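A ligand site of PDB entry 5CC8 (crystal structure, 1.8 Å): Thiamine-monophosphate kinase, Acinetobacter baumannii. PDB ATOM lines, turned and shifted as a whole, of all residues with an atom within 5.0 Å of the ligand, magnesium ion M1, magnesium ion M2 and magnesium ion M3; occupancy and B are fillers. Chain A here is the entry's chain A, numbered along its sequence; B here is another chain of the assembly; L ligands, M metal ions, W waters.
Water W5 lies within hydrogen-bond range of the backbone carbonyl oxygen of Ala 50 of chain B and the backbone carbonyl oxygen of Gly 125.
Water W11 lies within hydrogen-bond range of the side-chain carboxylate of Asp 206 of chain B (2.7 Å), the side-chain hydroxyl of Ser 208 of chain B (2.9 Å) and a nitrogen (N1) of the ligand (3.2 Å).
Water W8 lies within hydrogen-bond range of O of Asp 206 of chain B (2.8 Å) and OG of Ser 208 of chain B (3.3 Å).
Water W1 bridges an oxygen (O3) of the ligand and the side-chain carboxylate (OD2) of Asp 209 of chain B.
Water W15 bridges an oxygen (O6) of the ligand (2.8 Å) and the guanidinium group (NH1) of Arg 151 of chain B (3.1 Å).
Water W12 lies within hydrogen-bond range of N of Ala 50 of chain B (3.0 Å), O of Gly 125 (3.0 Å) and O12 of the ligand (3.3 Å).
Magnesium ion M2 is bound by O4 of the ligand (2.0 Å), OD1 of Asp 79 of chain B (2.0 Å), OD1 of Asp 206 of chain B (2.0 Å), OD1 of Asp 34 (2.1 Å), water W8 (2.1 Å) and water W11 (2.2 Å).
Two residues have an atom within 4 Å of magnesium ion M3: Asp 51 of chain B and Asp 79 of chain B.
O7 of the ligand binds magnesium ion M1 (2.1 Å).
OD1 of Asp 51 of chain B binds magnesium ion M1 (2.1 Å).
Magnesium ion M1 is bound by OD1 of Asp 126 (2.1 Å).
Water W5 is bound to magnesium ion M1, 2.1 Å away.
An oxygen (O1) of the ligand binds magnesium ion M1 (2.1 Å).
O5 of the ligand binds magnesium ion M1 (2.6 Å).
A nitrogen (N6) of the ligand sits close to the backbone carbonyl oxygen (O) of Gly 124.
CD1 of Ile 15 touches C6 of the ligand (3.4 Å).
Phe 19 touches the ligand.
Ile 31 touches the ligand.
O of Leu 92 touches N4 of the ligand, at 3.6 Å.
Of the 25 residues printed, 17 come within 4 Å of the ligand.
The nearest printed residue that does not touch the ligand is Leu 122 (4.02 Å).
The backbone NH of Ile 31 lies within hydrogen-bond range of the backbone carbonyl oxygen of Ile 123 (3.3 Å).
The backbone carbonyl oxygen of Asp 126 is in hydrogen-bond range of the backbone NH of Ile 94 (2.9 Å).
O of Leu 92 lies within hydrogen-bond range of N of Asp 126, at 2.9 Å.
The side-chain carboxylate (OD2) of Asp 34 is in salt-bridge range of the guanidinium group (NE) of Arg 151 of chain B.
NE of Arg 151 of chain B lies within salt-bridge range of OD1 of Asp 33, at 3.9 Å.
The backbone carbonyl oxygen of Gly 124 is in hydrogen-bond range of the backbone NH of Leu 92 (2.8 Å).
Of the 25 residues printed, 2 come within 4 Å of magnesium ion M1.
The nearest printed residue that does not touch magnesium ion M1 is Ala 50 of chain B (4.2 Å).
NH2 of Arg 151 of chain B touches magnesium ion M2 (3.7 Å).
Of the 25 residues printed, 4 come within 4 Å of magnesium ion M2.
The nearest printed residue that does not touch magnesium ion M2 is Ser 208 of chain B (4.3 Å).
The side-chain hydroxyl of Ser 208 of chain B sits at hydrogen-bond distance from an oxygen (O3) of the ligand.
The backbone NH of Gly 125 sits at hydrogen-bond distance from an oxygen (O12) of the ligand, 3.0 Å away.
The backbone NH (N) of Asp 126 is in hydrogen-bond range of a nitrogen (N3) of the ligand, 3.4 Å away.
O4 of the ligand sits close to NH2 of Arg 151 of chain B (3.0 Å).
The backbone carbonyl oxygen (O) of Asp 33 lies within hydrogen-bond range of an oxygen (O11) of the ligand.
An oxygen (O11) of the ligand lies within hydrogen-bond range of the backbone NH (N) of Asp 33 (3.2 Å).
The side-chain hydroxyl (OG1) of Thr 127 lies within hydrogen-bond range of a nitrogen (N3) of the ligand (2.9 Å).
The side-chain carboxylate (OD1) of Asp 209 of chain B lies close to an oxygen (O3) of the ligand (2.6 Å).
O11 of the ligand sits at hydrogen-bond distance from N of Gly 32 (2.9 Å).
The backbone carbonyl oxygen of Gly 125 is in hydrogen-bond range of an oxygen (O12) of the ligand (3.3 Å).
An oxygen (O2) of the ligand is bound to magnesium ion M3.
Magnesium ion M3 is bound by OD2 of Asp 51 of chain B.
Magnesium ion M3 is bound by the side-chain carboxylate (OD2) of Asp 79 of chain B, 2.1 Å away.
Water W10 is bound to magnesium ion M3 (2.1 Å).
Water W11 is bound to magnesium ion M3 (2.3 Å).
Magnesium ion M3 is bound by an oxygen (O5) of the ligand (2.3 Å).
Magnesium ion M3 has six donor atoms within binding distance.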
ATOM      1  N   ILE A  15      -8.179 -20.194   6.790  1.00  0.00           N
ATOM      2  CA  ILE A  15      -7.401 -20.345   5.556  1.00  0.00           C
ATOM      3  C   ILE A  15      -8.188 -19.825   4.368  1.00  0.00           C
ATOM      4  O   ILE A  15      -7.681 -19.057   3.561  1.00  0.00           O
ATOM      5  CB  ILE A  15      -6.975 -21.798   5.327  1.00  0.00           C
ATOM      6  CG1 ILE A  15      -6.090 -22.294   6.476  1.00  0.00           C
ATOM      7  CG2 ILE A  15      -6.205 -21.913   4.016  1.00  0.00           C
ATOM      8  CD1 ILE A  15      -6.161 -23.789   6.679  1.00  0.00           C
ATOM      9  N   PHE A  19      -6.395 -16.498   3.626  1.00  0.00           N
ATOM     10  CA  PHE A  19      -5.138 -16.943   3.012  1.00  0.00           C
ATOM     11  C   PHE A  19      -5.370 -17.817   1.805  1.00  0.00           C
ATOM     12  O   PHE A  19      -4.743 -18.868   1.680  1.00  0.00           O
ATOM     13  CB  PHE A  19      -4.287 -17.734   4.020  1.00  0.00           C
ATOM     14  CG  PHE A  19      -3.960 -16.968   5.253  1.00  0.00           C
ATOM     15  CD1 PHE A  19      -3.152 -15.837   5.187  1.00  0.00           C
ATOM     16  CD2 PHE A  19      -4.447 -17.363   6.491  1.00  0.00           C
ATOM     17  CE1 PHE A  19      -2.861 -15.119   6.323  1.00  0.00           C
ATOM     18  CE2 PHE A  19      -4.152 -16.653   7.631  1.00  0.00           C
ATOM     19  CZ  PHE A  19      -3.351 -15.523   7.542  1.00  0.00           C
ATOM     20  N   GLY A  30      -1.306 -24.714  -5.848  1.00  0.00           N
ATOM     21  CA  GLY A  30      -1.257 -23.927  -4.646  1.00  0.00           C
ATOM     22  C   GLY A  30      -2.079 -24.513  -3.533  1.00  0.00           C
ATOM     23  O   GLY A  30      -2.304 -25.734  -3.460  1.00  0.00           O
ATOM     24  N   ILE A  31      -2.568 -23.633  -2.671  1.00  0.00           N
ATOM     25  CA  ILE A  31      -3.258 -24.019  -1.446  1.00  0.00           C
ATOM     26  C   ILE A  31      -4.430 -24.964  -1.687  1.00  0.00           C
ATOM     27  O   ILE A  31      -5.244 -24.738  -2.594  1.00  0.00           O
ATOM     28  CB  ILE A  31      -3.729 -22.759  -0.706  1.00  0.00           C
ATOM     29  CG1 ILE A  31      -2.529 -21.982  -0.187  1.00  0.00           C
ATOM     30  CG2 ILE A  31      -4.702 -23.118   0.419  1.00  0.00           C
ATOM     31  CD1 ILE A  31      -2.854 -20.564   0.118  1.00  0.00           C
ATOM     32  N   GLY A  32      -4.507 -26.016  -0.884  1.00  0.00           N
ATOM     33  CA  GLY A  32      -5.684 -26.874  -0.857  1.00  0.00           C
ATOM     34  C   GLY A  32      -5.391 -28.361  -0.743  1.00  0.00           C
ATOM     35  O   GLY A  32      -6.279 -29.177  -0.491  1.00  0.00           O
ATOM     36  N   ASP A  33      -4.139 -28.719  -0.947  1.00  0.00           N
ATOM     37  CA  ASP A  33      -3.763 -30.118  -0.872  1.00  0.00           C
ATOM     38  C   ASP A  33      -2.727 -30.340   0.225  1.00  0.00           C
ATOM     39  O   ASP A  33      -2.318 -29.412   0.914  1.00  0.00           O
ATOM     40  CB  ASP A  33      -3.227 -30.600  -2.219  1.00  0.00           C
ATOM     41  CG  ASP A  33      -3.687 -31.998  -2.557  1.00  0.00           C
ATOM     42  OD1 ASP A  33      -3.274 -32.949  -1.869  1.00  0.00           O
ATOM     43  OD2 ASP A  33      -4.497 -32.138  -3.511  1.00  0.00           O
ATOM     44  N   ASP A  34      -2.261 -31.576   0.375  1.00  0.00           N
ATOM     45  CA  ASP A  34      -1.303 -31.853   1.439  1.00  0.00           C
ATOM     46  C   ASP A  34       0.041 -31.141   1.287  1.00  0.00           C
ATOM     47  O   ASP A  34       0.656 -30.746   2.285  1.00  0.00           O
ATOM     48  CB  ASP A  34      -1.095 -33.354   1.540  1.00  0.00           C
ATOM     49  CG  ASP A  34      -2.365 -34.056   1.909  1.00  0.00           C
ATOM     50  OD1 ASP A  34      -2.701 -34.062   3.109  1.00  0.00           O
ATOM     51  OD2 ASP A  34      -3.054 -34.565   0.990  1.00  0.00           O
ATOM     52  N   LEU A  92       3.339 -20.138   4.820  1.00  0.00           N
ATOM     53  CA  LEU A  92       3.040 -19.404   6.041  1.00  0.00           C
ATOM     54  C   LEU A  92       2.601 -20.323   7.179  1.00  0.00           C
ATOM     55  O   LEU A  92       1.527 -20.945   7.094  1.00  0.00           O
ATOM     56  CB  LEU A  92       1.944 -18.359   5.766  1.00  0.00           C
ATOM     57  CG  LEU A  92       1.374 -17.645   6.990  1.00  0.00           C
ATOM     58  CD1 LEU A  92       2.494 -16.873   7.712  1.00  0.00           C
ATOM     59  CD2 LEU A  92       0.251 -16.711   6.572  1.00  0.00           C
ATOM     60  N   ILE A  94       1.465 -20.219  11.022  1.00  0.00           N
ATOM     61  CA  ILE A  94       1.125 -19.314  12.100  1.00  0.00           C
ATOM     62  C   ILE A  94       0.487 -20.069  13.272  1.00  0.00           C
ATOM     63  O   ILE A  94      -0.362 -20.936  13.074  1.00  0.00           O
ATOM     64  CB  ILE A  94       0.210 -18.172  11.600  1.00  0.00           C
ATOM     65  CG1 ILE A  94      -0.183 -17.262  12.756  1.00  0.00           C
ATOM     66  CG2 ILE A  94      -1.026 -18.718  10.902  1.00  0.00           C
ATOM     67  CD1 ILE A  94      -0.433 -15.835  12.336  1.00  0.00           C
ATOM     68  N   LEU A 122       1.787 -16.848  -2.206  1.00  0.00           N
ATOM     69  CA  LEU A 122       1.572 -17.631  -0.997  1.00  0.00           C
ATOM     70  C   LEU A 122       0.922 -18.970  -1.390  1.00  0.00           C
ATOM     71  O   LEU A 122      -0.236 -18.997  -1.815  1.00  0.00           O
ATOM     72  CB  LEU A 122       0.700 -16.863   0.017  1.00  0.00           C
ATOM     73  CG  LEU A 122       0.218 -17.624   1.264  1.00  0.00           C
ATOM     74  CD1 LEU A 122       1.405 -18.147   2.064  1.00  0.00           C
ATOM     75  CD2 LEU A 122      -0.644 -16.742   2.166  1.00  0.00           C
ATOM     76  N   ILE A 123       1.661 -20.067  -1.251  1.00  0.00           N
ATOM     77  CA  ILE A 123       1.220 -21.322  -1.846  1.00  0.00           C
ATOM     78  C   ILE A 123       0.864 -22.400  -0.846  1.00  0.00           C
ATOM     79  O   ILE A 123       0.428 -23.484  -1.245  1.00  0.00           O
ATOM     80  CB  ILE A 123       2.277 -21.880  -2.821  1.00  0.00           C
ATOM     81  CG1 ILE A 123       3.558 -22.268  -2.078  1.00  0.00           C
ATOM     82  CG2 ILE A 123       2.586 -20.859  -3.897  1.00  0.00           C
ATOM     83  CD1 ILE A 123       4.543 -22.979  -2.983  1.00  0.00           C
ATOM     84  N   GLY A 124       1.036 -22.116   0.436  1.00  0.00           N
ATOM     85  CA  GLY A 124       0.739 -23.103   1.465  1.00  0.00           C
ATOM     86  C   GLY A 124       1.163 -22.659   2.843  1.00  0.00           C
ATOM     87  O   GLY A 124       1.631 -21.531   3.046  1.00  0.00           O
ATOM     88  N   GLY A 125       1.005 -23.563   3.809  1.00  0.00           N
ATOM     89  CA  GLY A 125       1.371 -23.275   5.175  1.00  0.00           C
ATOM     90  C   GLY A 125       0.633 -24.144   6.171  1.00  0.00           C
ATOM     91  O   GLY A 125       0.182 -25.239   5.824  1.00  0.00           O
ATOM     92  N   ASP A 126       0.523 -23.648   7.394  1.00  0.00           N
ATOM     93  CA  ASP A 126      -0.160 -24.375   8.459  1.00  0.00           C
ATOM     94  C   ASP A 126      -0.694 -23.357   9.445  1.00  0.00           C
ATOM     95  O   ASP A 126      -0.049 -22.353   9.737  1.00  0.00           O
ATOM     96  CB  ASP A 126       0.785 -25.353   9.165  1.00  0.00           C
ATOM     97  CG  ASP A 126       0.033 -26.346  10.058  1.00  0.00           C
ATOM     98  OD1 ASP A 126      -0.959 -26.939   9.603  1.00  0.00           O
ATOM     99  OD2 ASP A 126       0.438 -26.519  11.228  1.00  0.00           O
ATOM    100  N   THR A 127      -1.882 -23.630   9.959  1.00  0.00           N
ATOM    101  CA  THR A 127      -2.540 -22.718  10.877  1.00  0.00           C
ATOM    102  C   THR A 127      -2.885 -23.476  12.135  1.00  0.00           C
ATOM    103  O   THR A 127      -3.607 -24.462  12.095  1.00  0.00           O
ATOM    104  CB  THR A 127      -3.813 -22.121  10.247  1.00  0.00           C
ATOM    105  OG1 THR A 127      -3.492 -21.521   8.988  1.00  0.00           O
ATOM    106  CG2 THR A 127      -4.425 -21.090  11.161  1.00  0.00           C
ATOM    107  N   ALA B  50       4.563 -27.586   5.109  1.00  0.00           N
ATOM    108  CA  ALA B  50       5.042 -27.262   6.449  1.00  0.00           C
ATOM    109  C   ALA B  50       3.929 -27.511   7.468  1.00  0.00           C
ATOM    110  O   ALA B  50       2.748 -27.303   7.171  1.00  0.00           O
ATOM    111  CB  ALA B  50       5.531 -25.816   6.524  1.00  0.00           C
ATOM    112  N   ASP B  51       4.336 -27.983   8.640  1.00  0.00           N
ATOM    113  CA  ASP B  51       3.414 -28.296   9.727  1.00  0.00           C
ATOM    114  C   ASP B  51       4.068 -27.924  11.047  1.00  0.00           C
ATOM    115  O   ASP B  51       5.250 -28.190  11.262  1.00  0.00           O
ATOM    116  CB  ASP B  51       3.062 -29.800   9.743  1.00  0.00           C
ATOM    117  CG  ASP B  51       1.717 -30.080   9.094  1.00  0.00           C
ATOM    118  OD1 ASP B  51       0.808 -29.219   9.121  1.00  0.00           O
ATOM    119  OD2 ASP B  51       1.550 -31.206   8.577  1.00  0.00           O
ATOM    120  N   VAL B  75       5.602 -35.986  10.726  1.00  0.00           N
ATOM    121  CA  VAL B  75       4.275 -35.493  10.288  1.00  0.00           C
ATOM    122  C   VAL B  75       4.410 -34.707   8.987  1.00  0.00           C
ATOM    123  O   VAL B  75       3.447 -34.590   8.233  1.00  0.00           O
ATOM    124  CB  VAL B  75       3.578 -34.647  11.383  1.00  0.00           C
ATOM    125  CG1 VAL B  75       3.396 -35.478  12.637  1.00  0.00           C
ATOM    126  CG2 VAL B  75       4.355 -33.355  11.678  1.00  0.00           C
ATOM    127  N   ASP B  79       2.961 -35.646   4.717  1.00  0.00           N
ATOM    128  CA  ASP B  79       2.326 -34.813   3.683  1.00  0.00           C
ATOM    129  C   ASP B  79       3.046 -34.853   2.327  1.00  0.00           C
ATOM    130  O   ASP B  79       2.395 -34.643   1.294  1.00  0.00           O
ATOM    131  CB  ASP B  79       2.223 -33.363   4.160  1.00  0.00           C
ATOM    132  CG  ASP B  79       1.010 -33.141   5.017  1.00  0.00           C
ATOM    133  OD1 ASP B  79      -0.064 -33.632   4.618  1.00  0.00           O
ATOM    134  OD2 ASP B  79       1.131 -32.516   6.089  1.00  0.00           O
ATOM    135  N   ARG B 151      -6.028 -34.552  -3.812  1.00  0.00           N
ATOM    136  CA  ARG B 151      -7.224 -34.871  -3.028  1.00  0.00           C
ATOM    137  C   ARG B 151      -8.432 -34.932  -3.926  1.00  0.00           C
ATOM    138  O   ARG B 151      -9.446 -35.540  -3.595  1.00  0.00           O
ATOM    139  CB  ARG B 151      -7.448 -33.856  -1.919  1.00  0.00           C
ATOM    140  CG  ARG B 151      -6.376 -33.896  -0.835  1.00  0.00           C
ATOM    141  CD  ARG B 151      -6.670 -32.841   0.198  1.00  0.00           C
ATOM    142  NE  ARG B 151      -5.646 -32.833   1.255  1.00  0.00           N
ATOM    143  CZ  ARG B 151      -5.710 -32.053   2.324  1.00  0.00           C
ATOM    144  NH1 ARG B 151      -6.728 -31.196   2.447  1.00  0.00           N
ATOM    145  NH2 ARG B 151      -4.761 -32.118   3.245  1.00  0.00           N
ATOM    146  N   ILE B 205      -4.929 -38.720   0.790  1.00  0.00           N
ATOM    147  CA  ILE B 205      -4.685 -37.750   1.868  1.00  0.00           C
ATOM    148  C   ILE B 205      -4.050 -38.518   3.026  1.00  0.00           C
ATOM    149  O   ILE B 205      -4.304 -39.712   3.169  1.00  0.00           O
ATOM    150  CB  ILE B 205      -5.990 -37.055   2.306  1.00  0.00           C
ATOM    151  CG1 ILE B 205      -5.691 -35.882   3.254  1.00  0.00           C
ATOM    152  CG2 ILE B 205      -6.921 -38.045   2.999  1.00  0.00           C
ATOM    153  CD1 ILE B 205      -6.902 -34.987   3.477  1.00  0.00           C
ATOM    154  N   ASP B 206      -3.239 -37.868   3.841  1.00  0.00           N
ATOM    155  CA  ASP B 206      -2.754 -38.555   5.038  1.00  0.00           C
ATOM    156  C   ASP B 206      -3.711 -38.235   6.181  1.00  0.00           C
ATOM    157  O   ASP B 206      -4.283 -37.143   6.249  1.00  0.00           O
ATOM    158  CB  ASP B 206      -1.292 -38.190   5.400  1.00  0.00           C
ATOM    159  CG  ASP B 206      -1.113 -36.731   5.718  1.00  0.00           C
ATOM    160  OD1 ASP B 206      -1.744 -35.896   5.053  1.00  0.00           O
ATOM    161  OD2 ASP B 206      -0.297 -36.412   6.628  1.00  0.00           O
ATOM    162  N   SER B 208      -4.184 -37.189   9.408  1.00  0.00           N
ATOM    163  CA  SER B 208      -3.539 -36.481  10.510  1.00  0.00           C
ATOM    164  C   SER B 208      -4.554 -36.016  11.555  1.00  0.00           C
ATOM    165  O   SER B 208      -4.229 -35.879  12.729  1.00  0.00           O
ATOM    166  CB  SER B 208      -2.720 -35.295   9.991  1.00  0.00           C
ATOM    167  OG  SER B 208      -3.454 -34.522   9.049  1.00  0.00           O
ATOM    168  N   ASP B 209      -5.786 -35.760  11.121  1.00  0.00           N
ATOM    169  CA  ASP B 209      -6.795 -35.243  12.024  1.00  0.00           C
ATOM    170  C   ASP B 209      -7.848 -36.273  12.406  1.00  0.00           C
ATOM    171  O   ASP B 209      -8.430 -36.190  13.493  1.00  0.00           O
ATOM    172  CB  ASP B 209      -7.477 -34.025  11.418  1.00  0.00           C
ATOM    173  CG  ASP B 209      -6.678 -32.761  11.620  1.00  0.00           C
ATOM    174  OD1 ASP B 209      -6.151 -32.229  10.629  1.00  0.00           O
ATOM    175  OD2 ASP B 209      -6.574 -32.310  12.784  1.00  0.00           O
ATOM    176  N   TYR B 258      -1.457 -40.706  10.968  1.00  0.00           N
ATOM    177  CA  TYR B 258      -0.470 -40.523   9.892  1.00  0.00           C
ATOM    178  C   TYR B 258      -0.377 -41.757   9.000  1.00  0.00           C
ATOM    179  O   TYR B 258       0.693 -42.119   8.500  1.00  0.00           O
ATOM    180  CB  TYR B 258       0.884 -40.083  10.482  1.00  0.00           C
ATOM    181  CG  TYR B 258       0.703 -38.726  11.119  1.00  0.00           C
ATOM    182  CD1 TYR B 258       0.600 -37.578  10.341  1.00  0.00           C
ATOM    183  CD2 TYR B 258       0.520 -38.604  12.488  1.00  0.00           C
ATOM    184  CE1 TYR B 258       0.376 -36.346  10.909  1.00  0.00           C
ATOM    185  CE2 TYR B 258       0.289 -37.383  13.068  1.00  0.00           C
ATOM    186  CZ  TYR B 258       0.200 -36.256  12.278  1.00  0.00           C
ATOM    187  OH  TYR B 258      -0.035 -35.026  12.854  1.00  0.00           O
HETATM  188  P1  LIG L   1      -2.568 -31.272   9.306  1.00  0.00           P
HETATM  189  O1  LIG L   1      -2.198 -29.915   9.690  1.00  0.00           O
HETATM  190  O2  LIG L   1      -1.264 -32.147   9.357  1.00  0.00           O
HETATM  191  O3  LIG L   1      -3.644 -31.785  10.340  1.00  0.00           O
HETATM  192  P2  LIG L   1      -2.440 -30.940   6.430  1.00  0.00           P
HETATM  193  O4  LIG L   1      -2.556 -32.031   5.305  1.00  0.00           O
HETATM  194  O5  LIG L   1      -1.048 -30.637   6.732  1.00  0.00           O
HETATM  195  N1  LIG L   1      -3.209 -31.354   7.798  1.00  0.00           N
HETATM  196  P3  LIG L   1      -3.721 -28.342   6.547  1.00  0.00           P
HETATM  197  O6  LIG L   1      -5.101 -28.653   7.149  1.00  0.00           O
HETATM  198  O7  LIG L   1      -2.758 -27.843   7.557  1.00  0.00           O
HETATM  199  O8  LIG L   1      -3.174 -29.658   5.835  1.00  0.00           O
HETATM  200  O9  LIG L   1      -3.895 -27.214   5.437  1.00  0.00           O
HETATM  201  C1  LIG L   1      -4.848 -27.298   4.369  1.00  0.00           C
HETATM  202  C2  LIG L   1      -4.299 -26.515   3.204  1.00  0.00           C
HETATM  203  O10 LIG L   1      -4.201 -25.113   3.574  1.00  0.00           O
HETATM  204  C3  LIG L   1      -2.899 -26.934   2.760  1.00  0.00           C
HETATM  205  O11 LIG L   1      -2.817 -26.890   1.337  1.00  0.00           O
HETATM  206  C4  LIG L   1      -1.994 -25.911   3.457  1.00  0.00           C
HETATM  207  O12 LIG L   1      -0.782 -25.737   2.737  1.00  0.00           O
HETATM  208  C5  LIG L   1      -2.872 -24.655   3.437  1.00  0.00           C
HETATM  209  N2  LIG L   1      -2.624 -23.715   4.525  1.00  0.00           N
HETATM  210  C6  LIG L   1      -2.871 -23.908   5.856  1.00  0.00           C
HETATM  211  N3  LIG L   1      -2.642 -22.855   6.606  1.00  0.00           N
HETATM  212  C7  LIG L   1      -2.205 -21.902   5.697  1.00  0.00           C
HETATM  213  C8  LIG L   1      -1.836 -20.556   5.856  1.00  0.00           C
HETATM  214  N4  LIG L   1      -1.881 -19.895   7.016  1.00  0.00           N
HETATM  215  N5  LIG L   1      -1.460 -19.876   4.747  1.00  0.00           N
HETATM  216  C9  LIG L   1      -1.478 -20.504   3.569  1.00  0.00           C
HETATM  217  N6  LIG L   1      -1.821 -21.763   3.299  1.00  0.00           N
HETATM  218  C10 LIG L   1      -2.184 -22.409   4.415  1.00  0.00           C
HETATM  219 MG    MG M   1      -1.058 -28.658   8.371  1.00  0.00          MG
HETATM  220 MG    MG M   2      -2.013 -33.891   5.054  1.00  0.00          MG
HETATM  221 MG    MG M   3       0.002 -32.320   7.835  1.00  0.00          MG
HETATM  222  O   HOH W   1      -3.703 -31.919  12.886  1.00  0.00           O
HETATM  223  O   HOH W   2       0.312 -32.808  11.369  1.00  0.00           O
HETATM  224  O   HOH W   3      -0.842 -29.038  12.074  1.00  0.00           O
HETATM  225  O   HOH W   4      -0.169 -25.939  -0.008  1.00  0.00           O
HETATM  226  O   HOH W   5       0.177 -27.780   6.864  1.00  0.00           O
HETATM  227  O   HOH W   6      -3.649 -25.548   8.840  1.00  0.00           O
HETATM  228  O   HOH W   7      -5.845 -32.810   7.025  1.00  0.00           O
HETATM  229  O   HOH W   8      -3.930 -34.456   5.750  1.00  0.00           O
HETATM  230  O   HOH W   9      -1.569 -27.585  -1.737  1.00  0.00           O
HETATM  231  O   HOH W  10       1.006 -33.918   8.771  1.00  0.00           O
HETATM  232  O   HOH W  11      -1.386 -33.945   7.111  1.00  0.00           O
HETATM  233  O   HOH W  12       1.784 -27.191   4.157  1.00  0.00           O
HETATM  234  O   HOH W  13      -4.701 -28.725  10.899  1.00  0.00           O
HETATM  235  O   HOH W  14       2.099 -26.670   1.381  1.00  0.00           O
HETATM  236  O   HOH W  15      -6.424 -30.492   5.440  1.00  0.00           O
